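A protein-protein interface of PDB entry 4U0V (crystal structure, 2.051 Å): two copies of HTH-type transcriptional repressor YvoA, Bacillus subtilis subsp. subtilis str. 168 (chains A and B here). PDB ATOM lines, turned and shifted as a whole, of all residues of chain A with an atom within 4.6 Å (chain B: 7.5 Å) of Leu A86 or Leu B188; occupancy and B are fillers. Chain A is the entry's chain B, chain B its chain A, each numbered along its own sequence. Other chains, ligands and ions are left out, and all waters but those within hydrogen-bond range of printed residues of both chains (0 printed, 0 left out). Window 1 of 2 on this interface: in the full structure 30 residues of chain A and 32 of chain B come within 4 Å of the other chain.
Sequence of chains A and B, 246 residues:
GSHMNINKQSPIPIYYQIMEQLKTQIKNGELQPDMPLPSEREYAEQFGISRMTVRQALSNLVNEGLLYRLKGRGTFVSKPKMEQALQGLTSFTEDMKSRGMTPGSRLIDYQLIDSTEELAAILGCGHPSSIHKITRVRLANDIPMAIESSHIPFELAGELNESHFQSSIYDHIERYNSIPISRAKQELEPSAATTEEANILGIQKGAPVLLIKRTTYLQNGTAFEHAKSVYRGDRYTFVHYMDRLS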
ATOM      1  N   GLN A  84      21.344  31.964  22.851  1.00  0.00           N
ATOM      2  CA  GLN A  84      22.656  31.546  22.412  1.00  0.00           C
ATOM      3  C   GLN A  84      22.603  31.217  20.929  1.00  0.00           C
ATOM      4  O   GLN A  84      21.949  30.252  20.533  1.00  0.00           O
ATOM      5  CB  GLN A  84      23.107  30.328  23.214  1.00  0.00           C
ATOM      6  CG  GLN A  84      24.509  29.855  22.912  1.00  0.00           C
ATOM      7  CD  GLN A  84      25.557  30.864  23.349  1.00  0.00           C
ATOM      8  OE1 GLN A  84      25.371  31.569  24.342  1.00  0.00           O
ATOM      9  NE2 GLN A  84      26.666  30.936  22.608  1.00  0.00           N
ATOM     10  N   ALA A  85      23.282  32.018  20.116  1.00  0.00           N
ATOM     11  CA  ALA A  85      23.360  31.790  18.682  1.00  0.00           C
ATOM     12  C   ALA A  85      24.302  30.620  18.354  1.00  0.00           C
ATOM     13  O   ALA A  85      25.481  30.641  18.688  1.00  0.00           O
ATOM     14  CB  ALA A  85      23.815  33.062  17.972  1.00  0.00           C
ATOM     15  N   LEU A  86      23.776  29.610  17.676  1.00  0.00           N
ATOM     16  CA  LEU A  86      24.548  28.418  17.352  1.00  0.00           C
ATOM     17  C   LEU A  86      25.531  28.581  16.181  1.00  0.00           C
ATOM     18  O   LEU A  86      26.488  27.823  16.065  1.00  0.00           O
ATOM     19  CB  LEU A  86      23.596  27.264  17.047  1.00  0.00           C
ATOM     20  CG  LEU A  86      22.857  26.695  18.260  1.00  0.00           C
ATOM     21  CD1 LEU A  86      21.888  25.613  17.837  1.00  0.00           C
ATOM     22  CD2 LEU A  86      23.853  26.151  19.272  1.00  0.00           C
ATOM     23  N   GLN A  87      25.295  29.545  15.301  1.00  0.00           N
ATOM     24  CA  GLN A  87      26.112  29.640  14.093  1.00  0.00           C
ATOM     25  C   GLN A  87      27.411  30.429  14.311  1.00  0.00           C
ATOM     26  O   GLN A  87      28.355  30.294  13.546  1.00  0.00           O
ATOM     27  CB  GLN A  87      25.276  30.249  12.955  1.00  0.00           C
ATOM     28  CG  GLN A  87      24.378  29.204  12.243  1.00  0.00           C
ATOM     29  CD  GLN A  87      23.053  29.776  11.740  1.00  0.00           C
ATOM     30  OE1 GLN A  87      22.241  30.292  12.524  1.00  0.00           O
ATOM     31  NE2 GLN A  87      22.834  29.701  10.429  1.00  0.00           N
ATOM     32  N   GLY A  88      27.461  31.243  15.361  1.00  0.00           N
ATOM     33  CA  GLY A  88      28.639  32.039  15.643  1.00  0.00           C
ATOM     34  C   GLY A  88      29.612  31.317  16.567  1.00  0.00           C
ATOM     35  O   GLY A  88      29.291  30.993  17.712  1.00  0.00           O
ATOM     36  N   GLN A 186      29.240  21.045  15.515  1.00  0.00           N
ATOM     37  CA  GLN A 186      28.634  20.619  16.781  1.00  0.00           C
ATOM     38  C   GLN A 186      27.539  19.576  16.568  1.00  0.00           C
ATOM     39  O   GLN A 186      26.828  19.589  15.557  1.00  0.00           O
ATOM     40  CB  GLN A 186      28.059  21.808  17.572  1.00  0.00           C
ATOM     41  CG  GLN A 186      29.093  22.643  18.298  1.00  0.00           C
ATOM     42  CD  GLN A 186      28.525  23.586  19.355  1.00  0.00           C
ATOM     43  OE1 GLN A 186      29.202  23.888  20.334  1.00  0.00           O
ATOM     44  NE2 GLN A 186      27.295  24.086  19.150  1.00  0.00           N
ATOM     45  N   LEU A 188      24.227  17.968  18.751  1.00  0.00           N
ATOM     46  CA  LEU A 188      23.345  18.376  19.843  1.00  0.00           C
ATOM     47  C   LEU A 188      22.357  17.262  20.152  1.00  0.00           C
ATOM     48  O   LEU A 188      21.804  16.664  19.237  1.00  0.00           O
ATOM     49  CB  LEU A 188      22.549  19.647  19.459  1.00  0.00           C
ATOM     50  CG  LEU A 188      23.113  21.064  19.600  1.00  0.00           C
ATOM     51  CD1 LEU A 188      24.515  21.176  19.048  1.00  0.00           C
ATOM     52  CD2 LEU A 188      22.209  22.064  18.898  1.00  0.00           C
ATOM     53  N   THR A 237      18.190  29.498  25.572  1.00  0.00           N
ATOM     54  CA  THR A 237      17.439  29.254  24.363  1.00  0.00           C
ATOM     55  C   THR A 237      18.399  29.273  23.188  1.00  0.00           C
ATOM     56  O   THR A 237      19.010  30.292  22.879  1.00  0.00           O
ATOM     57  CB  THR A 237      16.329  30.303  24.158  1.00  0.00           C
ATOM     58  OG1 THR A 237      15.290  30.084  25.122  1.00  0.00           O
ATOM     59  CG2 THR A 237      15.751  30.175  22.767  1.00  0.00           C
ATOM     60  N   PHE A 238      18.541  28.140  22.524  1.00  0.00           N
ATOM     61  CA  PHE A 238      19.503  28.065  21.443  1.00  0.00           C
ATOM     62  C   PHE A 238      18.842  28.429  20.136  1.00  0.00           C
ATOM     63  O   PHE A 238      17.785  27.900  19.808  1.00  0.00           O
ATOM     64  CB  PHE A 238      20.124  26.674  21.390  1.00  0.00           C
ATOM     65  CG  PHE A 238      20.778  26.282  22.675  1.00  0.00           C
ATOM     66  CD1 PHE A 238      22.097  26.624  22.921  1.00  0.00           C
ATOM     67  CD2 PHE A 238      20.064  25.631  23.659  1.00  0.00           C
ATOM     68  CE1 PHE A 238      22.700  26.293  24.120  1.00  0.00           C
ATOM     69  CE2 PHE A 238      20.663  25.306  24.859  1.00  0.00           C
ATOM     70  CZ  PHE A 238      21.990  25.636  25.081  1.00  0.00           C
ATOM     71  N   VAL A 239      19.489  29.318  19.389  1.00  0.00           N
ATOM     72  CA  VAL A 239      18.909  29.888  18.178  1.00  0.00           C
ATOM     73  C   VAL A 239      19.801  29.674  16.979  1.00  0.00           C
ATOM     74  O   VAL A 239      21.033  29.759  17.084  1.00  0.00           O
ATOM     75  CB  VAL A 239      18.651  31.412  18.348  1.00  0.00           C
ATOM     76  CG1 VAL A 239      18.109  32.028  17.078  1.00  0.00           C
ATOM     77  CG2 VAL A 239      17.694  31.666  19.497  1.00  0.00           C
ATOM     78  N   HIS A 240      19.178  29.393  15.840  1.00  0.00           N
ATOM     79  CA  HIS A 240      19.892  29.333  14.582  1.00  0.00           C
ATOM     80  C   HIS A 240      18.939  29.692  13.456  1.00  0.00           C
ATOM     81  O   HIS A 240      17.730  29.855  13.666  1.00  0.00           O
ATOM     82  CB  HIS A 240      20.495  27.952  14.360  1.00  0.00           C
ATOM     83  CG  HIS A 240      19.472  26.888  14.156  1.00  0.00           C
ATOM     84  ND1 HIS A 240      19.070  26.467  12.903  1.00  0.00           N
ATOM     85  CD2 HIS A 240      18.718  26.197  15.044  1.00  0.00           C
ATOM     86  CE1 HIS A 240      18.135  25.543  13.030  1.00  0.00           C
ATOM     87  NE2 HIS A 240      17.900  25.363  14.321  1.00  0.00           N
ATOM     88  N   LEU B  86      20.850  21.121  10.893  1.00  0.00           N
ATOM     89  CA  LEU B  86      20.072  22.261  11.379  1.00  0.00           C
ATOM     90  C   LEU B  86      20.013  23.432  10.415  1.00  0.00           C
ATOM     91  O   LEU B  86      19.117  24.262  10.509  1.00  0.00           O
ATOM     92  CB  LEU B  86      20.633  22.762  12.707  1.00  0.00           C
ATOM     93  CG  LEU B  86      20.165  21.913  13.880  1.00  0.00           C
ATOM     94  CD1 LEU B  86      20.715  22.457  15.169  1.00  0.00           C
ATOM     95  CD2 LEU B  86      18.640  21.871  13.891  1.00  0.00           C
ATOM     96  N   GLN B  87      20.960  23.534   9.492  1.00  0.00           N
ATOM     97  CA  GLN B  87      21.014  24.759   8.701  1.00  0.00           C
ATOM     98  C   GLN B  87      20.268  24.688   7.369  1.00  0.00           C
ATOM     99  O   GLN B  87      19.936  25.721   6.794  1.00  0.00           O
ATOM    100  CB  GLN B  87      22.463  25.165   8.469  1.00  0.00           C
ATOM    101  CG  GLN B  87      23.089  25.793   9.704  1.00  0.00           C
ATOM    102  CD  GLN B  87      24.594  25.742   9.662  1.00  0.00           C
ATOM    103  OE1 GLN B  87      25.207  24.818  10.191  1.00  0.00           O
ATOM    104  NE2 GLN B  87      25.201  26.729   9.017  1.00  0.00           N
ATOM    105  N   GLN B 186      14.845  29.097  14.098  1.00  0.00           N
ATOM    106  CA  GLN B 186      14.458  28.080  15.082  1.00  0.00           C
ATOM    107  C   GLN B 186      15.026  28.363  16.466  1.00  0.00           C
ATOM    108  O   GLN B 186      16.141  28.873  16.611  1.00  0.00           O
ATOM    109  CB  GLN B 186      14.891  26.666  14.645  1.00  0.00           C
ATOM    110  CG  GLN B 186      14.064  26.085  13.532  1.00  0.00           C
ATOM    111  CD  GLN B 186      14.209  24.567  13.360  1.00  0.00           C
ATOM    112  OE1 GLN B 186      13.270  23.907  12.919  1.00  0.00           O
ATOM    113  NE2 GLN B 186      15.387  24.018  13.683  1.00  0.00           N
ATOM    114  N   GLU B 187      14.243  28.003  17.477  1.00  0.00           N
ATOM    115  CA  GLU B 187      14.642  28.075  18.869  1.00  0.00           C
ATOM    116  C   GLU B 187      14.574  26.683  19.443  1.00  0.00           C
ATOM    117  O   GLU B 187      13.546  26.018  19.342  1.00  0.00           O
ATOM    118  CB  GLU B 187      13.737  29.003  19.684  1.00  0.00           C
ATOM    119  CG  GLU B 187      13.934  30.487  19.443  1.00  0.00           C
ATOM    120  CD  GLU B 187      12.814  31.323  20.076  1.00  0.00           C
ATOM    121  OE1 GLU B 187      12.388  31.020  21.213  1.00  0.00           O
ATOM    122  OE2 GLU B 187      12.355  32.274  19.427  1.00  0.00           O
ATOM    123  N   LEU B 188      15.671  26.254  20.054  1.00  0.00           N
ATOM    124  CA  LEU B 188      15.818  24.890  20.538  1.00  0.00           C
ATOM    125  C   LEU B 188      15.924  24.910  22.048  1.00  0.00           C
ATOM    126  O   LEU B 188      16.587  25.764  22.618  1.00  0.00           O
ATOM    127  CB  LEU B 188      17.067  24.227  19.946  1.00  0.00           C
ATOM    128  CG  LEU B 188      17.255  24.320  18.444  1.00  0.00           C
ATOM    129  CD1 LEU B 188      18.561  23.715  17.996  1.00  0.00           C
ATOM    130  CD2 LEU B 188      16.109  23.610  17.798  1.00  0.00           C
ATOM    131  N   GLU B 189      15.284  23.946  22.684  1.00  0.00           N
ATOM    132  CA  GLU B 189      15.304  23.814  24.124  1.00  0.00           C
ATOM    133  C   GLU B 189      15.159  22.333  24.434  1.00  0.00           C
ATOM    134  O   GLU B 189      14.282  21.693  23.860  1.00  0.00           O
ATOM    135  CB  GLU B 189      14.157  24.620  24.749  1.00  0.00           C
ATOM    136  CG  GLU B 189      14.133  24.579  26.242  1.00  0.00           C
ATOM    137  CD  GLU B 189      13.196  25.603  26.839  1.00  0.00           C
ATOM    138  OE1 GLU B 189      13.064  25.612  28.083  1.00  0.00           O
ATOM    139  OE2 GLU B 189      12.584  26.373  26.062  1.00  0.00           O
ATOM    140  N   PRO B 190      16.031  21.770  25.303  1.00  0.00           N
ATOM    141  CA  PRO B 190      15.822  20.388  25.751  1.00  0.00           C
ATOM    142  C   PRO B 190      14.620  20.306  26.670  1.00  0.00           C
ATOM    143  O   PRO B 190      14.306  21.260  27.401  1.00  0.00           O
ATOM    144  CB  PRO B 190      17.114  20.051  26.510  1.00  0.00           C
ATOM    145  CG  PRO B 190      17.587  21.360  27.007  1.00  0.00           C
ATOM    146  CD  PRO B 190      17.238  22.356  25.914  1.00  0.00           C
ATOM    147  N   LEU B 210      13.736  17.151  22.199  1.00  0.00           N
ATOM    148  CA  LEU B 210      14.133  18.488  21.858  1.00  0.00           C
ATOM    149  C   LEU B 210      12.873  19.264  21.475  1.00  0.00           C
ATOM    150  O   LEU B 210      12.156  18.886  20.550  1.00  0.00           O
ATOM    151  CB  LEU B 210      15.143  18.503  20.719  1.00  0.00           C
ATOM    152  CG  LEU B 210      15.867  19.838  20.470  1.00  0.00           C
ATOM    153  CD1 LEU B 210      16.680  20.238  21.702  1.00  0.00           C
ATOM    154  CD2 LEU B 210      16.780  19.734  19.283  1.00  0.00           C
ATOM    155  N   LEU B 211      12.617  20.335  22.212  1.00  0.00           N
ATOM    156  CA  LEU B 211      11.503  21.243  21.935  1.00  0.00           C
ATOM    157  C   LEU B 211      11.955  22.310  20.931  1.00  0.00           C
ATOM    158  O   LEU B 211      12.861  23.083  21.213  1.00  0.00           O
ATOM    159  CB  LEU B 211      11.015  21.895  23.239  1.00  0.00           C
ATOM    160  CG  LEU B 211       9.897  22.938  23.109  1.00  0.00           C
ATOM    161  CD1 LEU B 211       8.710  22.368  22.324  1.00  0.00           C
ATOM    162  CD2 LEU B 211       9.450  23.415  24.483  1.00  0.00           C
ATOM    163  N   ILE B 212      11.339  22.347  19.754  1.00  0.00           N
ATOM    164  CA  ILE B 212      11.749  23.279  18.724  1.00  0.00           C
ATOM    165  C   ILE B 212      10.623  24.210  18.270  1.00  0.00           C
ATOM    166  O   ILE B 212       9.551  23.738  17.879  1.00  0.00           O
ATOM    167  CB  ILE B 212      12.275  22.549  17.478  1.00  0.00           C
ATOM    168  CG1 ILE B 212      13.361  21.525  17.871  1.00  0.00           C
ATOM    169  CG2 ILE B 212      12.775  23.574  16.459  1.00  0.00           C
ATOM    170  CD1 ILE B 212      14.054  20.881  16.679  1.00  0.00           C
ATOM    171  N   LYS B 213      10.882  25.517  18.309  1.00  0.00           N
ATOM    172  CA  LYS B 213       9.999  26.505  17.681  1.00  0.00           C
ATOM    173  C   LYS B 213      10.588  27.019  16.398  1.00  0.00           C
ATOM    174  O   LYS B 213      11.715  27.533  16.372  1.00  0.00           O
ATOM    175  CB  LYS B 213       9.731  27.697  18.603  1.00  0.00           C
ATOM    176  CG  LYS B 213       8.680  27.438  19.646  1.00  0.00           C
ATOM    177  CD  LYS B 213       8.287  28.739  20.348  1.00  0.00           C
ATOM    178  CE  LYS B 213       9.186  29.044  21.528  1.00  0.00           C
ATOM    179  NZ  LYS B 213       8.797  30.313  22.223  1.00  0.00           N
ATOM    180  N   TYR B 231      10.864  16.553  19.286  1.00  0.00           N
ATOM    181  CA  TYR B 231      11.576  15.472  18.605  1.00  0.00           C
ATOM    182  C   TYR B 231      12.147  14.476  19.603  1.00  0.00           C
ATOM    183  O   TYR B 231      12.743  14.877  20.591  1.00  0.00           O
ATOM    184  CB  TYR B 231      12.685  16.048  17.737  1.00  0.00           C
ATOM    185  CG  TYR B 231      12.185  16.676  16.466  1.00  0.00           C
ATOM    186  CD1 TYR B 231      12.265  15.989  15.268  1.00  0.00           C
ATOM    187  CD2 TYR B 231      11.610  17.947  16.464  1.00  0.00           C
ATOM    188  CE1 TYR B 231      11.803  16.535  14.101  1.00  0.00           C
ATOM    189  CE2 TYR B 231      11.147  18.506  15.286  1.00  0.00           C
ATOM    190  CZ  TYR B 231      11.243  17.782  14.114  1.00  0.00           C
ATOM    191  OH  TYR B 231      10.796  18.312  12.933  1.00  0.00           O
ATOM    192  N   PHE B 238      21.277  16.184  16.281  1.00  0.00           N
ATOM    193  CA  PHE B 238      21.171  17.433  15.555  1.00  0.00           C
ATOM    194  C   PHE B 238      22.551  18.013  15.302  1.00  0.00           C
ATOM    195  O   PHE B 238      23.341  18.198  16.221  1.00  0.00           O
ATOM    196  CB  PHE B 238      20.269  18.399  16.326  1.00  0.00           C
ATOM    197  CG  PHE B 238      18.872  17.888  16.454  1.00  0.00           C
ATOM    198  CD1 PHE B 238      17.953  18.077  15.434  1.00  0.00           C
ATOM    199  CD2 PHE B 238      18.510  17.122  17.540  1.00  0.00           C
ATOM    200  CE1 PHE B 238      16.676  17.564  15.529  1.00  0.00           C
ATOM    201  CE2 PHE B 238      17.218  16.607  17.640  1.00  0.00           C
ATOM    202  CZ  PHE B 238      16.313  16.824  16.616  1.00  0.00           C
ATOM    203  N   HIS B 240      25.101  20.938  13.419  1.00  0.00           N
ATOM    204  CA  HIS B 240      25.285  22.205  12.729  1.00  0.00           C
ATOM    205  C   HIS B 240      26.749  22.601  12.664  1.00  0.00           C
ATOM    206  O   HIS B 240      27.620  21.915  13.212  1.00  0.00           O
ATOM    207  CB  HIS B 240      24.478  23.302  13.397  1.00  0.00           C
ATOM    208  CG  HIS B 240      25.011  23.703  14.726  1.00  0.00           C
ATOM    209  ND1 HIS B 240      25.903  24.744  14.889  1.00  0.00           N
ATOM    210  CD2 HIS B 240      24.800  23.189  15.961  1.00  0.00           C
ATOM    211  CE1 HIS B 240      26.206  24.864  16.171  1.00  0.00           C
ATOM    212  NE2 HIS B 240      25.545  23.938  16.843  1.00  0.00           N
ATOM    213  N   TYR B 241      27.017  23.708  11.975  1.00  0.00           N
ATOM    214  CA  TYR B 241      28.371  24.213  11.864  1.00  0.00           C
ATOM    215  C   TYR B 241      28.436  25.654  12.368  1.00  0.00           C
ATOM    216  O   TYR B 241      27.411  26.325  12.526  1.00  0.00           O
ATOM    217  CB  TYR B 241      28.867  24.098  10.417  1.00  0.00           C
ATOM    218  CG  TYR B 241      28.972  22.668   9.937  1.00  0.00           C
ATOM    219  CD1 TYR B 241      30.178  21.982   9.998  1.00  0.00           C
ATOM    220  CD2 TYR B 241      27.857  21.995   9.437  1.00  0.00           C
ATOM    221  CE1 TYR B 241      30.279  20.668   9.564  1.00  0.00           C
ATOM    222  CE2 TYR B 241      27.948  20.682   9.003  1.00  0.00           C
ATOM    223  CZ  TYR B 241      29.160  20.024   9.071  1.00  0.00           C
ATOM    224  OH  TYR B 241      29.256  18.719   8.651  1.00  0.00           O
ATOM    225  N   MET B 242      29.647  26.111  12.663  1.00  0.00           N
ATOM    226  CA  MET B 242      29.854  27.447  13.196  1.00  0.00           C
ATOM    227  C   MET B 242      31.052  28.088  12.523  1.00  0.00           C
ATOM    228  O   MET B 242      31.964  27.385  12.100  1.00  0.00           O
ATOM    229  CB  MET B 242      30.087  27.411  14.708  1.00  0.00           C
ATOM    230  CG  MET B 242      29.357  26.310  15.469  1.00  0.00           C
ATOM    231  SD  MET B 242      29.900  26.208  17.200  1.00  0.00           S
ATOM    232  CE  MET B 242      29.123  27.658  17.901  1.00  0.00           C
ATOM    233  N   ASP B 243      31.061  29.415  12.427  1.00  0.00           N
ATOM    234  CA  ASP B 243      32.297  30.105  12.065  1.00  0.00           C
ATOM    235  C   ASP B 243      32.323  31.488  12.686  1.00  0.00           C
ATOM    236  O   ASP B 243      31.396  31.858  13.402  1.00  0.00           O
ATOM    237  CB  ASP B 243      32.486  30.175  10.540  1.00  0.00           C
ATOM    238  CG  ASP B 243      31.272  30.698   9.811  1.00  0.00           C
ATOM    239  OD1 ASP B 243      31.000  30.180   8.709  1.00  0.00           O
ATOM    240  OD2 ASP B 243      30.603  31.627  10.318  1.00  0.00           O
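NE2 of His B240 sits at hydrogen-bond distance from NE2 of Gln A186, 2.9 Å away.
NE2 of Gln B186 is in hydrogen-bond range of NE2 of His A240, at 2.9 Å.
The backbone carbonyl oxygen (O) of Gln A87 is in hydrogen-bond range of the backbone NH (N) of Asp B243, 3.1 Å away.
ND1 of His B240 lies close to O of Leu A86 (3.3 Å).
The backbone carbonyl oxygen (O) of Leu B86 lies close to a ring nitrogen (ND1) of His A240.
N of Leu A188 is in hydrogen-bond range of O of Phe B238 (2.7 Å).
The backbone carbonyl oxygen (O) of Phe A238 lies within hydrogen-bond range of the backbone NH (N) of Leu B188, 2.7 Å away.
O of Val A239 lies within hydrogen-bond range of N of Leu A86 (2.8 Å).
OE1 of Glu B187 lies within salt-bridge range of NZ of Lys B213.
N of Gln A84 lies within hydrogen-bond range of O of Thr A237, 2.9 Å away.
The backbone carbonyl oxygen (O) of Gln A84 is in hydrogen-bond range of the backbone NH (N) of Val A239, 2.9 Å away.
The backbone NH (N) of Tyr B241 is in hydrogen-bond range of the side-chain amide oxygen (OE1) of Gln B87, at 2.8 Å.
Leu A86 touches Leu B188 (CD1 to CD1, 3.8 Å).
Leu A86 touches Tyr B241 (O to O, 3.95 Å).
O of Tyr B241 touches CA of Gln A87, 3.9 Å away.
Met B242 touches Gly A88.
CA of Gly A88 touches O of Asp B243, at 3.6 Å.
CD of Gln A186 touches SD of Met B242, at 3.7 Å.
Leu A188 touches His B240 (CD1 to NE2, 3.7 Å).
Thr A237 touches Glu B187.
Phe A238 touches Gln B186.
CD1 of Leu B188 touches CD2 of His A240, 3.9 Å away.
Of chain B, only Leu B188 (3.8 Å), His B240 (3.0 Å), Tyr B241 (3.95 Å) and Met B242 (3.2 Å) come within 4 Å of Leu A86.
Of the printed residues of chain B, Gln A87 touches Gln B87 (3.98 Å), Tyr B241 (3.9 Å), Met B242 (3.2 Å) and Asp B243 (3.1 Å).
Printed residues of chain B within 4 Å of Leu A188: Phe B238 (2.7 Å) and His B240 (3.7 Å).
Printed residues of chain A within 4 Å of Leu B86: His A240 (3.0 Å).
Of the printed residues of chain A, Leu B188 touches Leu A86, Thr A237, Phe A238 and His A240.
Of the printed residues of chain A, Tyr B241 touches Leu A86 (3.95 Å) and Gln A87 (3.9 Å).
The nearest printed residue of chain A that does not touch Glu B187 is His A240 (5.4 Å).
Hydrophobic or aromatic side chains of chain B that line the printed part of chain A: Leu B86, Leu B188, Phe B238, His B240 and Met B242.
Printed residues of chain A that touch a printed residue of chain B: Leu A86, Gln A87, Gly A88, Gln A186, Leu A188, Thr A237, Phe A238, Val A239 and His A240.
Among the printed residues, no Asp or Glu carboxylate lies within 4 Å of a Lys or Arg side-chain nitrogen of the other chain.
Leu A86 touches Leu B188, but with the chains exchanged Leu A188 does not touch Leu B86 (4.04 Å).
Gln B87 touches its own counterpart, Gln A87.
Gln A186 touches His B240, and with the chains exchanged His A240 touches Gln B186.
Leu A188 touches Phe B238, and with the chains exchanged Phe A238 touches Leu B188.
Positions printed for both chains: 86, 87, 186, 188, 238 and 240.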
